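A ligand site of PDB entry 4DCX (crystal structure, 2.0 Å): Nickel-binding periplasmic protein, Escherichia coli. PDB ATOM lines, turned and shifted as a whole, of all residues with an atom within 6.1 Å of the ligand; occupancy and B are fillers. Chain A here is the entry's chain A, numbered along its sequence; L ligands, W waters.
The guanidinium group of Arg 137 sits close to the side-chain sulfur of Met 27 (3.8 Å). The indole nitrogen (NE1) of Trp 100 sits at hydrogen-bond distance from the side-chain hydroxyl (OH) of Tyr 22.
CD1 of Tyr 22 touches O1 of the ligand (3.5 Å). Thr 23 touches the ligand (CG2 to C21, 3.1 Å). Met 27 touches the ligand. Trp 100 touches the ligand (CG to C2, 3.2 Å). Trp 398 touches the ligand. Tyr 402 touches the ligand. CG2 of Thr 490 touches C12 of the ligand, at 3.4 Å. Hydrophobic or aromatic side chains that line the ligand: Tyr 22, Met 27, Trp 100, Trp 398, Tyr 402 and His 416. The nearest printed residue that does not touch the ligand is Ser 415 (4.04 Å).
Water W3 lies within hydrogen-bond range of the backbone carbonyl oxygen (O) of Arg 137 (2.7 Å), the side-chain hydroxyl (OH) of Tyr 402 (2.8 Å) and an oxygen (O2) of the ligand (2.8 Å). Water W1 bridges O4 of the ligand (2.8 Å) and OH of Tyr 382 (3.1 Å).
The guanidinium group of Arg 137 lies within salt-bridge range of an oxygen (O2) of the ligand (3.0 Å). An oxygen (O4) of the ligand is in hydrogen-bond range of a ring nitrogen (NE2) of His 416 (3.0 Å).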
ATOM      1  N   TYR A  22     -13.641  11.132  19.097  1.00  0.00           N
ATOM      2  CA  TYR A  22     -13.597  10.137  18.041  1.00  0.00           C
ATOM      3  C   TYR A  22     -14.451   8.918  18.437  1.00  0.00           C
ATOM      4  O   TYR A  22     -15.636   9.076  18.723  1.00  0.00           O
ATOM      5  CB  TYR A  22     -12.139   9.793  17.722  1.00  0.00           C
ATOM      6  CG  TYR A  22     -11.347  11.026  17.295  1.00  0.00           C
ATOM      7  CD1 TYR A  22     -11.289  11.401  15.955  1.00  0.00           C
ATOM      8  CD2 TYR A  22     -10.684  11.821  18.226  1.00  0.00           C
ATOM      9  CE1 TYR A  22     -10.590  12.535  15.548  1.00  0.00           C
ATOM     10  CE2 TYR A  22      -9.972  12.960  17.836  1.00  0.00           C
ATOM     11  CZ  TYR A  22      -9.932  13.308  16.487  1.00  0.00           C
ATOM     12  OH  TYR A  22      -9.242  14.428  16.084  1.00  0.00           O
ATOM     13  N   THR A  23     -13.888   7.715  18.450  1.00  0.00           N
ATOM     14  CA  THR A  23     -14.653   6.539  18.866  1.00  0.00           C
ATOM     15  C   THR A  23     -15.283   6.786  20.223  1.00  0.00           C
ATOM     16  O   THR A  23     -14.655   7.360  21.109  1.00  0.00           O
ATOM     17  CB  THR A  23     -13.753   5.322  19.041  1.00  0.00           C
ATOM     18  OG1 THR A  23     -12.909   5.511  20.184  1.00  0.00           O
ATOM     19  CG2 THR A  23     -12.915   5.126  17.829  1.00  0.00           C
ATOM     20  N   MET A  27     -18.924   9.263  12.589  1.00  0.00           N
ATOM     21  CA  MET A  27     -18.735  10.522  11.883  1.00  0.00           C
ATOM     22  C   MET A  27     -19.968  11.008  11.118  1.00  0.00           C
ATOM     23  O   MET A  27     -20.265  12.207  11.108  1.00  0.00           O
ATOM     24  CB  MET A  27     -17.548  10.436  10.924  1.00  0.00           C
ATOM     25  CG  MET A  27     -16.232  10.236  11.653  1.00  0.00           C
ATOM     26  SD  MET A  27     -14.816  10.101  10.546  1.00  0.00           S
ATOM     27  CE  MET A  27     -14.601  11.792   9.970  1.00  0.00           C
ATOM     28  N   ARG A  97      -4.982  15.059  21.453  1.00  0.00           N
ATOM     29  CA  ARG A  97      -5.716  14.034  20.728  1.00  0.00           C
ATOM     30  C   ARG A  97      -5.937  14.417  19.253  1.00  0.00           C
ATOM     31  O   ARG A  97      -6.283  13.574  18.422  1.00  0.00           O
ATOM     32  CB  ARG A  97      -7.065  13.793  21.400  1.00  0.00           C
ATOM     33  CG  ARG A  97      -7.268  12.372  21.928  1.00  0.00           C
ATOM     34  CD  ARG A  97      -6.274  12.031  23.034  1.00  0.00           C
ATOM     35  NE  ARG A  97      -4.991  11.595  22.493  1.00  0.00           N
ATOM     36  CZ  ARG A  97      -3.839  11.607  23.184  1.00  0.00           C
ATOM     37  NH1 ARG A  97      -3.828  12.039  24.439  1.00  0.00           N
ATOM     38  NH2 ARG A  97      -2.712  11.196  22.605  1.00  0.00           N
ATOM     39  N   TRP A 100      -2.694  14.874  14.947  1.00  0.00           N
ATOM     40  CA  TRP A 100      -2.565  14.332  13.603  1.00  0.00           C
ATOM     41  C   TRP A 100      -3.030  15.367  12.581  1.00  0.00           C
ATOM     42  O   TRP A 100      -2.606  15.333  11.415  1.00  0.00           O
ATOM     43  CB  TRP A 100      -3.428  13.074  13.470  1.00  0.00           C
ATOM     44  CG  TRP A 100      -4.881  13.367  13.678  1.00  0.00           C
ATOM     45  CD1 TRP A 100      -5.546  13.401  14.875  1.00  0.00           C
ATOM     46  CD2 TRP A 100      -5.848  13.666  12.671  1.00  0.00           C
ATOM     47  NE1 TRP A 100      -6.874  13.713  14.668  1.00  0.00           N
ATOM     48  CE2 TRP A 100      -7.087  13.872  13.321  1.00  0.00           C
ATOM     49  CE3 TRP A 100      -5.795  13.777  11.274  1.00  0.00           C
ATOM     50  CZ2 TRP A 100      -8.246  14.196  12.626  1.00  0.00           C
ATOM     51  CZ3 TRP A 100      -6.953  14.101  10.579  1.00  0.00           C
ATOM     52  CH2 TRP A 100      -8.167  14.302  11.263  1.00  0.00           C
ATOM     53  N   ARG A 137     -15.183  16.566  12.071  1.00  0.00           N
ATOM     54  CA  ARG A 137     -14.711  16.764  13.438  1.00  0.00           C
ATOM     55  C   ARG A 137     -13.216  17.099  13.379  1.00  0.00           C
ATOM     56  O   ARG A 137     -12.539  16.704  12.438  1.00  0.00           O
ATOM     57  CB  ARG A 137     -15.004  15.510  14.306  1.00  0.00           C
ATOM     58  CG  ARG A 137     -14.265  14.228  13.866  1.00  0.00           C
ATOM     59  CD  ARG A 137     -14.913  12.970  14.448  1.00  0.00           C
ATOM     60  NE  ARG A 137     -14.179  11.738  14.120  1.00  0.00           N
ATOM     61  CZ  ARG A 137     -14.581  10.513  14.465  1.00  0.00           C
ATOM     62  NH1 ARG A 137     -15.721  10.329  15.119  1.00  0.00           N
ATOM     63  NH2 ARG A 137     -13.841   9.466  14.142  1.00  0.00           N
ATOM     64  N   PRO A 138     -12.705  17.812  14.386  1.00  0.00           N
ATOM     65  CA  PRO A 138     -13.387  18.199  15.617  1.00  0.00           C
ATOM     66  C   PRO A 138     -13.956  19.625  15.645  1.00  0.00           C
ATOM     67  O   PRO A 138     -14.533  19.991  16.666  1.00  0.00           O
ATOM     68  CB  PRO A 138     -12.267  18.127  16.643  1.00  0.00           C
ATOM     69  CG  PRO A 138     -11.065  18.579  15.875  1.00  0.00           C
ATOM     70  CD  PRO A 138     -11.264  18.105  14.452  1.00  0.00           C
ATOM     71  N   GLU A 247     -11.105   7.202  -2.710  1.00  0.00           N
ATOM     72  CA  GLU A 247      -9.853   7.032  -1.964  1.00  0.00           C
ATOM     73  C   GLU A 247      -9.127   5.740  -2.323  1.00  0.00           C
ATOM     74  O   GLU A 247      -9.665   4.888  -3.009  1.00  0.00           O
ATOM     75  CB  GLU A 247     -10.137   7.082  -0.463  1.00  0.00           C
ATOM     76  CG  GLU A 247     -10.965   5.915   0.020  1.00  0.00           C
ATOM     77  CD  GLU A 247     -11.756   6.216   1.285  1.00  0.00           C
ATOM     78  OE1 GLU A 247     -12.243   5.258   1.918  1.00  0.00           O
ATOM     79  OE2 GLU A 247     -11.930   7.399   1.635  1.00  0.00           O
ATOM     80  N   TYR A 382      -4.590  -1.573  15.603  1.00  0.00           N
ATOM     81  CA  TYR A 382      -4.266  -0.177  15.847  1.00  0.00           C
ATOM     82  C   TYR A 382      -2.949  -0.075  16.615  1.00  0.00           C
ATOM     83  O   TYR A 382      -2.120   0.803  16.328  1.00  0.00           O
ATOM     84  CB  TYR A 382      -5.400   0.527  16.587  1.00  0.00           C
ATOM     85  CG  TYR A 382      -6.614   0.755  15.713  1.00  0.00           C
ATOM     86  CD1 TYR A 382      -6.548   0.565  14.329  1.00  0.00           C
ATOM     87  CD2 TYR A 382      -7.837   1.152  16.265  1.00  0.00           C
ATOM     88  CE1 TYR A 382      -7.658   0.772  13.525  1.00  0.00           C
ATOM     89  CE2 TYR A 382      -8.947   1.357  15.477  1.00  0.00           C
ATOM     90  CZ  TYR A 382      -8.855   1.163  14.110  1.00  0.00           C
ATOM     91  OH  TYR A 382      -9.969   1.377  13.318  1.00  0.00           O
ATOM     92  N   GLN A 385      -0.079  -0.522  14.156  1.00  0.00           N
ATOM     93  CA  GLN A 385       0.119   0.694  13.392  1.00  0.00           C
ATOM     94  C   GLN A 385       1.015   1.647  14.178  1.00  0.00           C
ATOM     95  O   GLN A 385       1.956   2.219  13.620  1.00  0.00           O
ATOM     96  CB  GLN A 385      -1.213   1.400  13.125  1.00  0.00           C
ATOM     97  CG  GLN A 385      -2.211   0.629  12.284  1.00  0.00           C
ATOM     98  CD  GLN A 385      -3.520   1.388  12.151  1.00  0.00           C
ATOM     99  OE1 GLN A 385      -3.678   2.481  12.699  1.00  0.00           O
ATOM    100  NE2 GLN A 385      -4.473   0.817  11.416  1.00  0.00           N
ATOM    101  N   THR A 397      -6.283   5.638   2.171  1.00  0.00           N
ATOM    102  CA  THR A 397      -6.258   7.080   2.321  1.00  0.00           C
ATOM    103  C   THR A 397      -7.633   7.578   2.745  1.00  0.00           C
ATOM    104  O   THR A 397      -8.542   6.779   2.998  1.00  0.00           O
ATOM    105  CB  THR A 397      -5.731   7.791   1.044  1.00  0.00           C
ATOM    106  OG1 THR A 397      -6.674   7.616  -0.013  1.00  0.00           O
ATOM    107  CG2 THR A 397      -4.361   7.224   0.658  1.00  0.00           C
ATOM    108  N   TRP A 398      -7.807   8.899   2.857  1.00  0.00           N
ATOM    109  CA  TRP A 398      -8.953   9.410   3.601  1.00  0.00           C
ATOM    110  C   TRP A 398     -10.009  10.113   2.753  1.00  0.00           C
ATOM    111  O   TRP A 398     -11.049  10.498   3.280  1.00  0.00           O
ATOM    112  CB  TRP A 398      -8.491  10.316   4.739  1.00  0.00           C
ATOM    113  CG  TRP A 398      -7.609   9.599   5.753  1.00  0.00           C
ATOM    114  CD1 TRP A 398      -7.522   8.257   5.956  1.00  0.00           C
ATOM    115  CD2 TRP A 398      -6.699  10.212   6.681  1.00  0.00           C
ATOM    116  NE1 TRP A 398      -6.622   7.995   6.976  1.00  0.00           N
ATOM    117  CE2 TRP A 398      -6.102   9.171   7.430  1.00  0.00           C
ATOM    118  CE3 TRP A 398      -6.331  11.538   6.962  1.00  0.00           C
ATOM    119  CZ2 TRP A 398      -5.156   9.418   8.415  1.00  0.00           C
ATOM    120  CZ3 TRP A 398      -5.397  11.779   7.946  1.00  0.00           C
ATOM    121  CH2 TRP A 398      -4.814  10.721   8.659  1.00  0.00           C
ATOM    122  N   GLY A 399      -9.755  10.245   1.457  1.00  0.00           N
ATOM    123  CA  GLY A 399     -10.712  10.885   0.570  1.00  0.00           C
ATOM    124  C   GLY A 399     -10.777  12.373   0.786  1.00  0.00           C
ATOM    125  O   GLY A 399     -10.042  12.912   1.629  1.00  0.00           O
ATOM    126  N   TYR A 402      -9.363  15.488   2.905  1.00  0.00           N
ATOM    127  CA  TYR A 402      -8.114  15.070   3.579  1.00  0.00           C
ATOM    128  C   TYR A 402      -6.943  14.785   2.618  1.00  0.00           C
ATOM    129  O   TYR A 402      -5.784  15.034   2.955  1.00  0.00           O
ATOM    130  CB  TYR A 402      -8.359  13.776   4.358  1.00  0.00           C
ATOM    131  CG  TYR A 402      -9.446  13.834   5.397  1.00  0.00           C
ATOM    132  CD1 TYR A 402     -10.762  13.517   5.080  1.00  0.00           C
ATOM    133  CD2 TYR A 402      -9.151  14.145   6.721  1.00  0.00           C
ATOM    134  CE1 TYR A 402     -11.763  13.537   6.047  1.00  0.00           C
ATOM    135  CE2 TYR A 402     -10.135  14.164   7.693  1.00  0.00           C
ATOM    136  CZ  TYR A 402     -11.440  13.858   7.342  1.00  0.00           C
ATOM    137  OH  TYR A 402     -12.421  13.871   8.302  1.00  0.00           O
ATOM    138  N   SER A 410      -0.305  13.738   8.589  1.00  0.00           N
ATOM    139  CA  SER A 410      -0.413  12.643   9.547  1.00  0.00           C
ATOM    140  C   SER A 410       0.762  11.663   9.504  1.00  0.00           C
ATOM    141  O   SER A 410       0.990  10.917  10.467  1.00  0.00           O
ATOM    142  CB  SER A 410      -1.709  11.873   9.258  1.00  0.00           C
ATOM    143  OG  SER A 410      -1.834  10.714  10.056  1.00  0.00           O
ATOM    144  N   SER A 415       0.298   7.333  14.705  1.00  0.00           N
ATOM    145  CA  SER A 415      -1.092   7.009  15.036  1.00  0.00           C
ATOM    146  C   SER A 415      -1.631   6.094  13.946  1.00  0.00           C
ATOM    147  O   SER A 415      -2.166   5.006  14.208  1.00  0.00           O
ATOM    148  CB  SER A 415      -1.943   8.280  15.146  1.00  0.00           C
ATOM    149  OG  SER A 415      -3.281   7.978  15.512  1.00  0.00           O
ATOM    150  N   HIS A 416      -1.494   6.539  12.700  1.00  0.00           N
ATOM    151  CA  HIS A 416      -1.677   5.617  11.597  1.00  0.00           C
ATOM    152  C   HIS A 416      -0.300   5.012  11.334  1.00  0.00           C
ATOM    153  O   HIS A 416       0.684   5.410  11.964  1.00  0.00           O
ATOM    154  CB  HIS A 416      -2.267   6.293  10.352  1.00  0.00           C
ATOM    155  CG  HIS A 416      -3.770   6.328  10.360  1.00  0.00           C
ATOM    156  ND1 HIS A 416      -4.487   7.208  11.149  1.00  0.00           N
ATOM    157  CD2 HIS A 416      -4.678   5.557   9.720  1.00  0.00           C
ATOM    158  CE1 HIS A 416      -5.782   6.995  10.966  1.00  0.00           C
ATOM    159  NE2 HIS A 416      -5.926   5.997  10.109  1.00  0.00           N
ATOM    160  N   THR A 490     -17.247  10.535   4.317  1.00  0.00           N
ATOM    161  CA  THR A 490     -17.819   9.992   5.529  1.00  0.00           C
ATOM    162  C   THR A 490     -19.206  10.537   5.809  1.00  0.00           C
ATOM    163  O   THR A 490     -19.865  10.116   6.766  1.00  0.00           O
ATOM    164  CB  THR A 490     -16.936  10.284   6.749  1.00  0.00           C
ATOM    165  OG1 THR A 490     -16.758  11.695   6.867  1.00  0.00           O
ATOM    166  CG2 THR A 490     -15.581   9.639   6.587  1.00  0.00           C
HETATM  167  C1  LIG L   1      -6.176  10.334  11.939  1.00  0.00           C
HETATM  168  C2  LIG L   1      -5.702  10.319  13.243  1.00  0.00           C
HETATM  169  C3  LIG L   1      -6.562  10.002  14.291  1.00  0.00           C
HETATM  170  C4  LIG L   1      -7.887   9.717  14.013  1.00  0.00           C
HETATM  171  N1  LIG L   1      -8.310   9.751  12.762  1.00  0.00           N
HETATM  172  C5  LIG L   1      -7.519  10.063  11.721  1.00  0.00           C
HETATM  173  C6  LIG L   1      -8.137  10.054  10.325  1.00  0.00           C
HETATM  174  N2  LIG L   1      -9.522   9.858  10.655  1.00  0.00           N
HETATM  175  C7  LIG L   1     -10.017  11.188  11.139  1.00  0.00           C
HETATM  176  C8  LIG L   1     -11.263  11.130  12.075  1.00  0.00           C
HETATM  177  O1  LIG L   1     -11.501  10.062  12.697  1.00  0.00           O
HETATM  178  O2  LIG L   1     -11.885  12.204  12.257  1.00  0.00           O
HETATM  179  C9  LIG L   1     -10.154   9.266   9.464  1.00  0.00           C
HETATM  180  C10 LIG L   1     -10.391  10.342   8.381  1.00  0.00           C
HETATM  181  C11 LIG L   1     -11.055   9.672   7.193  1.00  0.00           C
HETATM  182  C12 LIG L   1     -12.400   9.057   7.612  1.00  0.00           C
HETATM  183  C13 LIG L   1     -12.136   8.020   8.717  1.00  0.00           C
HETATM  184  C14 LIG L   1     -11.475   8.725   9.904  1.00  0.00           C
HETATM  185  N3  LIG L   1     -11.212   7.709  10.958  1.00  0.00           N
HETATM  186  C15 LIG L   1     -10.529   6.562  10.322  1.00  0.00           C
HETATM  187  C16 LIG L   1      -9.199   6.215  11.026  1.00  0.00           C
HETATM  188  O3  LIG L   1      -8.679   7.066  11.788  1.00  0.00           O
HETATM  189  O4  LIG L   1      -8.692   5.107  10.756  1.00  0.00           O
HETATM  190  C17 LIG L   1     -12.454   7.236  11.573  1.00  0.00           C
HETATM  191  C18 LIG L   1     -12.041   6.587  12.886  1.00  0.00           C
HETATM  192  C19 LIG L   1     -12.683   5.460  13.385  1.00  0.00           C
HETATM  193  C20 LIG L   1     -12.245   4.924  14.589  1.00  0.00           C
HETATM  194  C21 LIG L   1     -11.205   5.562  15.277  1.00  0.00           C
HETATM  195  C22 LIG L   1     -10.621   6.697  14.734  1.00  0.00           C
HETATM  196  N4  LIG L   1     -11.056   7.162  13.579  1.00  0.00           N
HETATM  197 FE1  LIG L   1      -9.993   8.618  12.316  1.00  0.00          FE
HETATM  198  O   HOH W   1      -9.424   2.415  10.463  1.00  0.00           O
HETATM  199  O   HOH W   2     -13.185   3.962  10.297  1.00  0.00           O
HETATM  200  O   HOH W   3     -11.896  14.638  10.905  1.00  0.00           O
HETATM  201  O   HOH W   4      -9.776   5.466   7.128  1.00  0.00           O
